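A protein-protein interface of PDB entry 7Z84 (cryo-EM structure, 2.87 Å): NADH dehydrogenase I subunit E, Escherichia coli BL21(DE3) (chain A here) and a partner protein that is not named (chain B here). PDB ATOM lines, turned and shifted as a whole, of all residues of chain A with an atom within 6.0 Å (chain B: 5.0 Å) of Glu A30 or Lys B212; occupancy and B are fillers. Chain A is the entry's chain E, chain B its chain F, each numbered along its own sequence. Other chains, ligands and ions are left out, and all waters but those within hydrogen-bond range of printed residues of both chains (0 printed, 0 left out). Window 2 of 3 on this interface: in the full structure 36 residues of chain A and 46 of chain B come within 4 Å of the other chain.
Glu A30 touches just these residues of chain B: Tyr B86, Arg B127, Trp B210 and Lys B212. Of the printed residues of chain B, Asp A31 touches Trp B210. Of the printed residues of chain A, Arg B127 touches His A28, Tyr A29 and Glu A30. Of the printed residues of chain A, Tyr B86 touches Glu A30. Of the printed residues of chain A, Trp B210 touches Tyr A29 (3.9 Å), Glu A30 (3.4 Å) and Asp A31 (3.4 Å).
Printed residues of chain A that touch a printed residue of chain B: His A28, Tyr A29, Glu A30 and Asp A31. Hydrophobic or aromatic side chains of chain A within 4 Å of the printed part of chain B: Tyr A29. Among the printed residues, Asp or Glu carboxylates within 4 Å of a Lys or Arg side-chain nitrogen of the other chain: Glu A30 with Lys B212 (3.7 Å).
Among the printed residues, merely in contact across the chains: His A28 with Arg B127 (3.6 Å), Tyr A29 with Arg B127 (3.996 Å), Tyr A29 with Tyr B129 (3.6 Å), Tyr A29 with Trp B210 (3.9 Å), Glu A30 with Arg B127 (3.9 Å), Glu A30 with Trp B210 (3.4 Å) and Asp A31 with Trp B210 (3.4 Å).
The side-chain hydroxyl (OH) of Tyr B86 sits at hydrogen-bond distance from the side-chain carboxylate (OE2) of Glu A30 (2.5 Å). OE1 of Glu A30 lies within salt-bridge range of NZ of Lys B212 (3.7 Å). The backbone carbonyl oxygen of His A28 is in hydrogen-bond range of the side-chain hydroxyl of Tyr B129 (2.8 Å).
The backbone NH (N) of Tyr B86 sits at hydrogen-bond distance from the backbone carbonyl oxygen (O) of Pro B213 (3.0 Å). O of Lys B212 lies within hydrogen-bond range of OG1 of Thr B214, at 3.0 Å. The backbone carbonyl oxygen (O) of Trp B210 lies within hydrogen-bond range of the side-chain amino group (NZ) of Lys B212 (2.9 Å).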
ATOM      1  N   MET A  26     -31.169  16.642   6.736  1.00  0.00           N
ATOM      2  CA  MET A  26     -30.582  17.639   7.637  1.00  0.00           C
ATOM      3  C   MET A  26     -31.584  18.178   8.648  1.00  0.00           C
ATOM      4  O   MET A  26     -31.170  18.807   9.627  1.00  0.00           O
ATOM      5  CB  MET A  26     -29.950  18.821   6.888  1.00  0.00           C
ATOM      6  CG  MET A  26     -29.365  18.528   5.534  1.00  0.00           C
ATOM      7  SD  MET A  26     -28.349  19.874   4.902  1.00  0.00           S
ATOM      8  CE  MET A  26     -29.546  21.200   4.844  1.00  0.00           C
ATOM      9  N   HIS A  27     -32.885  17.960   8.438  1.00  0.00           N
ATOM     10  CA  HIS A  27     -33.852  18.266   9.488  1.00  0.00           C
ATOM     11  C   HIS A  27     -33.669  17.394  10.729  1.00  0.00           C
ATOM     12  O   HIS A  27     -34.061  17.809  11.824  1.00  0.00           O
ATOM     13  CB  HIS A  27     -35.280  18.105   8.966  1.00  0.00           C
ATOM     14  CG  HIS A  27     -35.731  19.220   8.076  1.00  0.00           C
ATOM     15  ND1 HIS A  27     -36.811  19.106   7.229  1.00  0.00           N
ATOM     16  CD2 HIS A  27     -35.250  20.474   7.906  1.00  0.00           C
ATOM     17  CE1 HIS A  27     -36.976  20.240   6.573  1.00  0.00           C
ATOM     18  NE2 HIS A  27     -36.041  21.087   6.965  1.00  0.00           N
ATOM     19  N   HIS A  28     -33.079  16.205  10.584  1.00  0.00           N
ATOM     20  CA  HIS A  28     -32.995  15.248  11.681  1.00  0.00           C
ATOM     21  C   HIS A  28     -31.877  15.553  12.670  1.00  0.00           C
ATOM     22  O   HIS A  28     -31.873  14.983  13.767  1.00  0.00           O
ATOM     23  CB  HIS A  28     -32.793  13.836  11.129  1.00  0.00           C
ATOM     24  CG  HIS A  28     -33.960  13.313  10.353  1.00  0.00           C
ATOM     25  ND1 HIS A  28     -35.143  14.008  10.225  1.00  0.00           N
ATOM     26  CD2 HIS A  28     -34.121  12.166   9.652  1.00  0.00           C
ATOM     27  CE1 HIS A  28     -35.985  13.309   9.486  1.00  0.00           C
ATOM     28  NE2 HIS A  28     -35.388  12.186   9.125  1.00  0.00           N
ATOM     29  N   TYR A  29     -30.934  16.422  12.320  1.00  0.00           N
ATOM     30  CA  TYR A  29     -29.760  16.659  13.148  1.00  0.00           C
ATOM     31  C   TYR A  29     -29.631  18.141  13.468  1.00  0.00           C
ATOM     32  O   TYR A  29     -30.211  18.998  12.798  1.00  0.00           O
ATOM     33  CB  TYR A  29     -28.480  16.168  12.461  1.00  0.00           C
ATOM     34  CG  TYR A  29     -28.586  14.782  11.871  1.00  0.00           C
ATOM     35  CD1 TYR A  29     -28.441  13.654  12.668  1.00  0.00           C
ATOM     36  CD2 TYR A  29     -28.822  14.601  10.515  1.00  0.00           C
ATOM     37  CE1 TYR A  29     -28.534  12.386  12.131  1.00  0.00           C
ATOM     38  CE2 TYR A  29     -28.917  13.338   9.970  1.00  0.00           C
ATOM     39  CZ  TYR A  29     -28.772  12.233  10.782  1.00  0.00           C
ATOM     40  OH  TYR A  29     -28.865  10.971  10.242  1.00  0.00           O
ATOM     41  N   GLU A  30     -28.854  18.430  14.512  1.00  0.00           N
ATOM     42  CA  GLU A  30     -28.566  19.806  14.895  1.00  0.00           C
ATOM     43  C   GLU A  30     -27.397  20.400  14.122  1.00  0.00           C
ATOM     44  O   GLU A  30     -27.137  21.601  14.249  1.00  0.00           O
ATOM     45  CB  GLU A  30     -28.283  19.887  16.397  1.00  0.00           C
ATOM     46  CG  GLU A  30     -27.115  19.035  16.860  1.00  0.00           C
ATOM     47  CD  GLU A  30     -26.492  19.553  18.140  1.00  0.00           C
ATOM     48  OE1 GLU A  30     -25.555  20.374  18.058  1.00  0.00           O
ATOM     49  OE2 GLU A  30     -26.942  19.141  19.229  1.00  0.00           O
ATOM     50  N   ASP A  31     -26.693  19.593  13.331  1.00  0.00           N
ATOM     51  CA  ASP A  31     -25.606  20.056  12.484  1.00  0.00           C
ATOM     52  C   ASP A  31     -25.866  19.538  11.075  1.00  0.00           C
ATOM     53  O   ASP A  31     -26.113  18.333  10.896  1.00  0.00           O
ATOM     54  CB  ASP A  31     -24.251  19.559  13.012  1.00  0.00           C
ATOM     55  CG  ASP A  31     -23.078  20.386  12.510  1.00  0.00           C
ATOM     56  OD1 ASP A  31     -23.031  20.720  11.310  1.00  0.00           O
ATOM     57  OD2 ASP A  31     -22.190  20.704  13.328  1.00  0.00           O
ATOM     58  N   PRO A  32     -25.847  20.406  10.057  1.00  0.00           N
ATOM     59  CA  PRO A  32     -26.058  19.929   8.678  1.00  0.00           C
ATOM     60  C   PRO A  32     -24.963  19.006   8.164  1.00  0.00           C
ATOM     61  O   PRO A  32     -25.197  18.305   7.175  1.00  0.00           O
ATOM     62  CB  PRO A  32     -26.119  21.227   7.859  1.00  0.00           C
ATOM     63  CG  PRO A  32     -25.507  22.273   8.734  1.00  0.00           C
ATOM     64  CD  PRO A  32     -25.836  21.875  10.133  1.00  0.00           C
ATOM     65  N   ILE B  84     -29.767  19.442  26.651  1.00  0.00           N
ATOM     66  CA  ILE B  84     -29.656  18.691  25.405  1.00  0.00           C
ATOM     67  C   ILE B  84     -28.852  17.425  25.665  1.00  0.00           C
ATOM     68  O   ILE B  84     -27.681  17.492  26.052  1.00  0.00           O
ATOM     69  CB  ILE B  84     -29.005  19.543  24.307  1.00  0.00           C
ATOM     70  CG1 ILE B  84     -29.878  20.758  23.984  1.00  0.00           C
ATOM     71  CG2 ILE B  84     -28.749  18.710  23.067  1.00  0.00           C
ATOM     72  CD1 ILE B  84     -31.264  20.399  23.505  1.00  0.00           C
ATOM     73  N   TYR B  86     -28.284  13.050  24.402  1.00  0.00           N
ATOM     74  CA  TYR B  86     -28.420  12.091  23.317  1.00  0.00           C
ATOM     75  C   TYR B  86     -28.250  10.668  23.828  1.00  0.00           C
ATOM     76  O   TYR B  86     -27.378  10.389  24.657  1.00  0.00           O
ATOM     77  CB  TYR B  86     -27.397  12.372  22.214  1.00  0.00           C
ATOM     78  CG  TYR B  86     -27.665  13.655  21.466  1.00  0.00           C
ATOM     79  CD1 TYR B  86     -28.743  13.765  20.602  1.00  0.00           C
ATOM     80  CD2 TYR B  86     -26.842  14.761  21.631  1.00  0.00           C
ATOM     81  CE1 TYR B  86     -28.994  14.936  19.919  1.00  0.00           C
ATOM     82  CE2 TYR B  86     -27.086  15.938  20.952  1.00  0.00           C
ATOM     83  CZ  TYR B  86     -28.164  16.019  20.099  1.00  0.00           C
ATOM     84  OH  TYR B  86     -28.411  17.187  19.418  1.00  0.00           O
ATOM     85  N   ARG B 127     -32.951  13.407  22.647  1.00  0.00           N
ATOM     86  CA  ARG B 127     -32.995  12.747  21.347  1.00  0.00           C
ATOM     87  C   ARG B 127     -32.333  11.379  21.404  1.00  0.00           C
ATOM     88  O   ARG B 127     -31.450  11.125  22.230  1.00  0.00           O
ATOM     89  CB  ARG B 127     -32.331  13.587  20.254  1.00  0.00           C
ATOM     90  CG  ARG B 127     -33.318  14.235  19.299  1.00  0.00           C
ATOM     91  CD  ARG B 127     -32.605  15.054  18.239  1.00  0.00           C
ATOM     92  NE  ARG B 127     -33.543  15.785  17.397  1.00  0.00           N
ATOM     93  CZ  ARG B 127     -33.215  16.820  16.637  1.00  0.00           C
ATOM     94  NH1 ARG B 127     -31.975  17.274  16.586  1.00  0.00           N
ATOM     95  NH2 ARG B 127     -34.156  17.415  15.909  1.00  0.00           N
ATOM     96  N   TYR B 129     -30.828   8.142  18.744  1.00  0.00           N
ATOM     97  CA  TYR B 129     -30.451   7.662  17.424  1.00  0.00           C
ATOM     98  C   TYR B 129     -30.078   6.191  17.509  1.00  0.00           C
ATOM     99  O   TYR B 129     -29.385   5.775  18.438  1.00  0.00           O
ATOM    100  CB  TYR B 129     -29.273   8.459  16.852  1.00  0.00           C
ATOM    101  CG  TYR B 129     -29.567   9.921  16.612  1.00  0.00           C
ATOM    102  CD1 TYR B 129     -30.055  10.358  15.388  1.00  0.00           C
ATOM    103  CD2 TYR B 129     -29.344  10.867  17.604  1.00  0.00           C
ATOM    104  CE1 TYR B 129     -30.320  11.694  15.163  1.00  0.00           C
ATOM    105  CE2 TYR B 129     -29.606  12.204  17.387  1.00  0.00           C
ATOM    106  CZ  TYR B 129     -30.095  12.611  16.165  1.00  0.00           C
ATOM    107  OH  TYR B 129     -30.358  13.942  15.942  1.00  0.00           O
ATOM    108  N   PRO B 204     -17.811  10.002  26.451  1.00  0.00           N
ATOM    109  CA  PRO B 204     -19.013  10.554  25.801  1.00  0.00           C
ATOM    110  C   PRO B 204     -20.106  10.997  26.758  1.00  0.00           C
ATOM    111  O   PRO B 204     -20.950  11.810  26.361  1.00  0.00           O
ATOM    112  CB  PRO B 204     -19.488   9.397  24.919  1.00  0.00           C
ATOM    113  CG  PRO B 204     -18.245   8.676  24.581  1.00  0.00           C
ATOM    114  CD  PRO B 204     -17.399   8.734  25.820  1.00  0.00           C
ATOM    115  N   THR B 206     -19.676  12.904  29.317  1.00  0.00           N
ATOM    116  CA  THR B 206     -19.394  14.307  29.592  1.00  0.00           C
ATOM    117  C   THR B 206     -19.549  15.165  28.339  1.00  0.00           C
ATOM    118  O   THR B 206     -20.229  16.196  28.369  1.00  0.00           O
ATOM    119  CB  THR B 206     -17.984  14.442  30.185  1.00  0.00           C
ATOM    120  OG1 THR B 206     -18.026  14.125  31.582  1.00  0.00           O
ATOM    121  CG2 THR B 206     -17.442  15.856  30.020  1.00  0.00           C
ATOM    122  N   SER B 207     -18.948  14.741  27.225  1.00  0.00           N
ATOM    123  CA  SER B 207     -19.034  15.492  25.973  1.00  0.00           C
ATOM    124  C   SER B 207     -18.977  14.484  24.829  1.00  0.00           C
ATOM    125  O   SER B 207     -17.892  14.035  24.448  1.00  0.00           O
ATOM    126  CB  SER B 207     -17.914  16.520  25.872  1.00  0.00           C
ATOM    127  OG  SER B 207     -16.655  15.888  25.738  1.00  0.00           O
ATOM    128  N   GLY B 208     -20.143  14.136  24.293  1.00  0.00           N
ATOM    129  CA  GLY B 208     -20.229  13.128  23.256  1.00  0.00           C
ATOM    130  C   GLY B 208     -20.654  13.653  21.902  1.00  0.00           C
ATOM    131  O   GLY B 208     -19.851  14.249  21.178  1.00  0.00           O
ATOM    132  N   ALA B 209     -21.918  13.436  21.550  1.00  0.00           N
ATOM    133  CA  ALA B 209     -22.422  13.801  20.232  1.00  0.00           C
ATOM    134  C   ALA B 209     -22.646  15.305  20.162  1.00  0.00           C
ATOM    135  O   ALA B 209     -23.447  15.853  20.928  1.00  0.00           O
ATOM    136  CB  ALA B 209     -23.713  13.046  19.928  1.00  0.00           C
ATOM    137  N   TRP B 210     -21.931  15.961  19.241  1.00  0.00           N
ATOM    138  CA  TRP B 210     -21.969  17.414  19.036  1.00  0.00           C
ATOM    139  C   TRP B 210     -21.638  18.183  20.312  1.00  0.00           C
ATOM    140  O   TRP B 210     -22.183  19.260  20.559  1.00  0.00           O
ATOM    141  CB  TRP B 210     -23.319  17.868  18.470  1.00  0.00           C
ATOM    142  CG  TRP B 210     -23.653  17.242  17.152  1.00  0.00           C
ATOM    143  CD1 TRP B 210     -23.154  17.589  15.932  1.00  0.00           C
ATOM    144  CD2 TRP B 210     -24.564  16.163  16.919  1.00  0.00           C
ATOM    145  NE1 TRP B 210     -23.692  16.790  14.956  1.00  0.00           N
ATOM    146  CE2 TRP B 210     -24.562  15.905  15.536  1.00  0.00           C
ATOM    147  CE3 TRP B 210     -25.380  15.387  17.748  1.00  0.00           C
ATOM    148  CZ2 TRP B 210     -25.344  14.907  14.963  1.00  0.00           C
ATOM    149  CZ3 TRP B 210     -26.152  14.395  17.177  1.00  0.00           C
ATOM    150  CH2 TRP B 210     -26.130  14.165  15.798  1.00  0.00           C
ATOM    151  N   GLY B 211     -20.740  17.635  21.132  1.00  0.00           N
ATOM    152  CA  GLY B 211     -20.338  18.266  22.368  1.00  0.00           C
ATOM    153  C   GLY B 211     -21.300  18.097  23.520  1.00  0.00           C
ATOM    154  O   GLY B 211     -20.971  18.502  24.642  1.00  0.00           O
ATOM    155  N   LYS B 212     -22.466  17.521  23.288  1.00  0.00           N
ATOM    156  CA  LYS B 212     -23.496  17.350  24.296  1.00  0.00           C
ATOM    157  C   LYS B 212     -23.303  16.037  25.037  1.00  0.00           C
ATOM    158  O   LYS B 212     -22.624  15.132  24.545  1.00  0.00           O
ATOM    159  CB  LYS B 212     -24.873  17.390  23.640  1.00  0.00           C
ATOM    160  CG  LYS B 212     -25.052  18.551  22.681  1.00  0.00           C
ATOM    161  CD  LYS B 212     -24.953  19.879  23.407  1.00  0.00           C
ATOM    162  CE  LYS B 212     -25.268  21.038  22.482  1.00  0.00           C
ATOM    163  NZ  LYS B 212     -24.252  21.174  21.405  1.00  0.00           N
ATOM    164  N   PRO B 213     -23.847  15.924  26.248  1.00  0.00           N
ATOM    165  CA  PRO B 213     -23.827  14.634  26.950  1.00  0.00           C
ATOM    166  C   PRO B 213     -24.557  13.545  26.171  1.00  0.00           C
ATOM    167  O   PRO B 213     -25.694  13.721  25.717  1.00  0.00           O
ATOM    168  CB  PRO B 213     -24.514  14.941  28.287  1.00  0.00           C
ATOM    169  CG  PRO B 213     -24.847  16.408  28.269  1.00  0.00           C
ATOM    170  CD  PRO B 213     -24.077  17.042  27.175  1.00  0.00           C
ATOM    171  N   THR B 214     -23.881  12.407  26.026  1.00  0.00           N
ATOM    172  CA  THR B 214     -24.306  11.330  25.150  1.00  0.00           C
ATOM    173  C   THR B 214     -24.034   9.998  25.831  1.00  0.00           C
ATOM    174  O   THR B 214     -22.981   9.813  26.444  1.00  0.00           O
ATOM    175  CB  THR B 214     -23.562  11.402  23.808  1.00  0.00           C
ATOM    176  OG1 THR B 214     -23.724  12.708  23.245  1.00  0.00           O
ATOM    177  CG2 THR B 214     -24.101  10.385  22.834  1.00  0.00           C
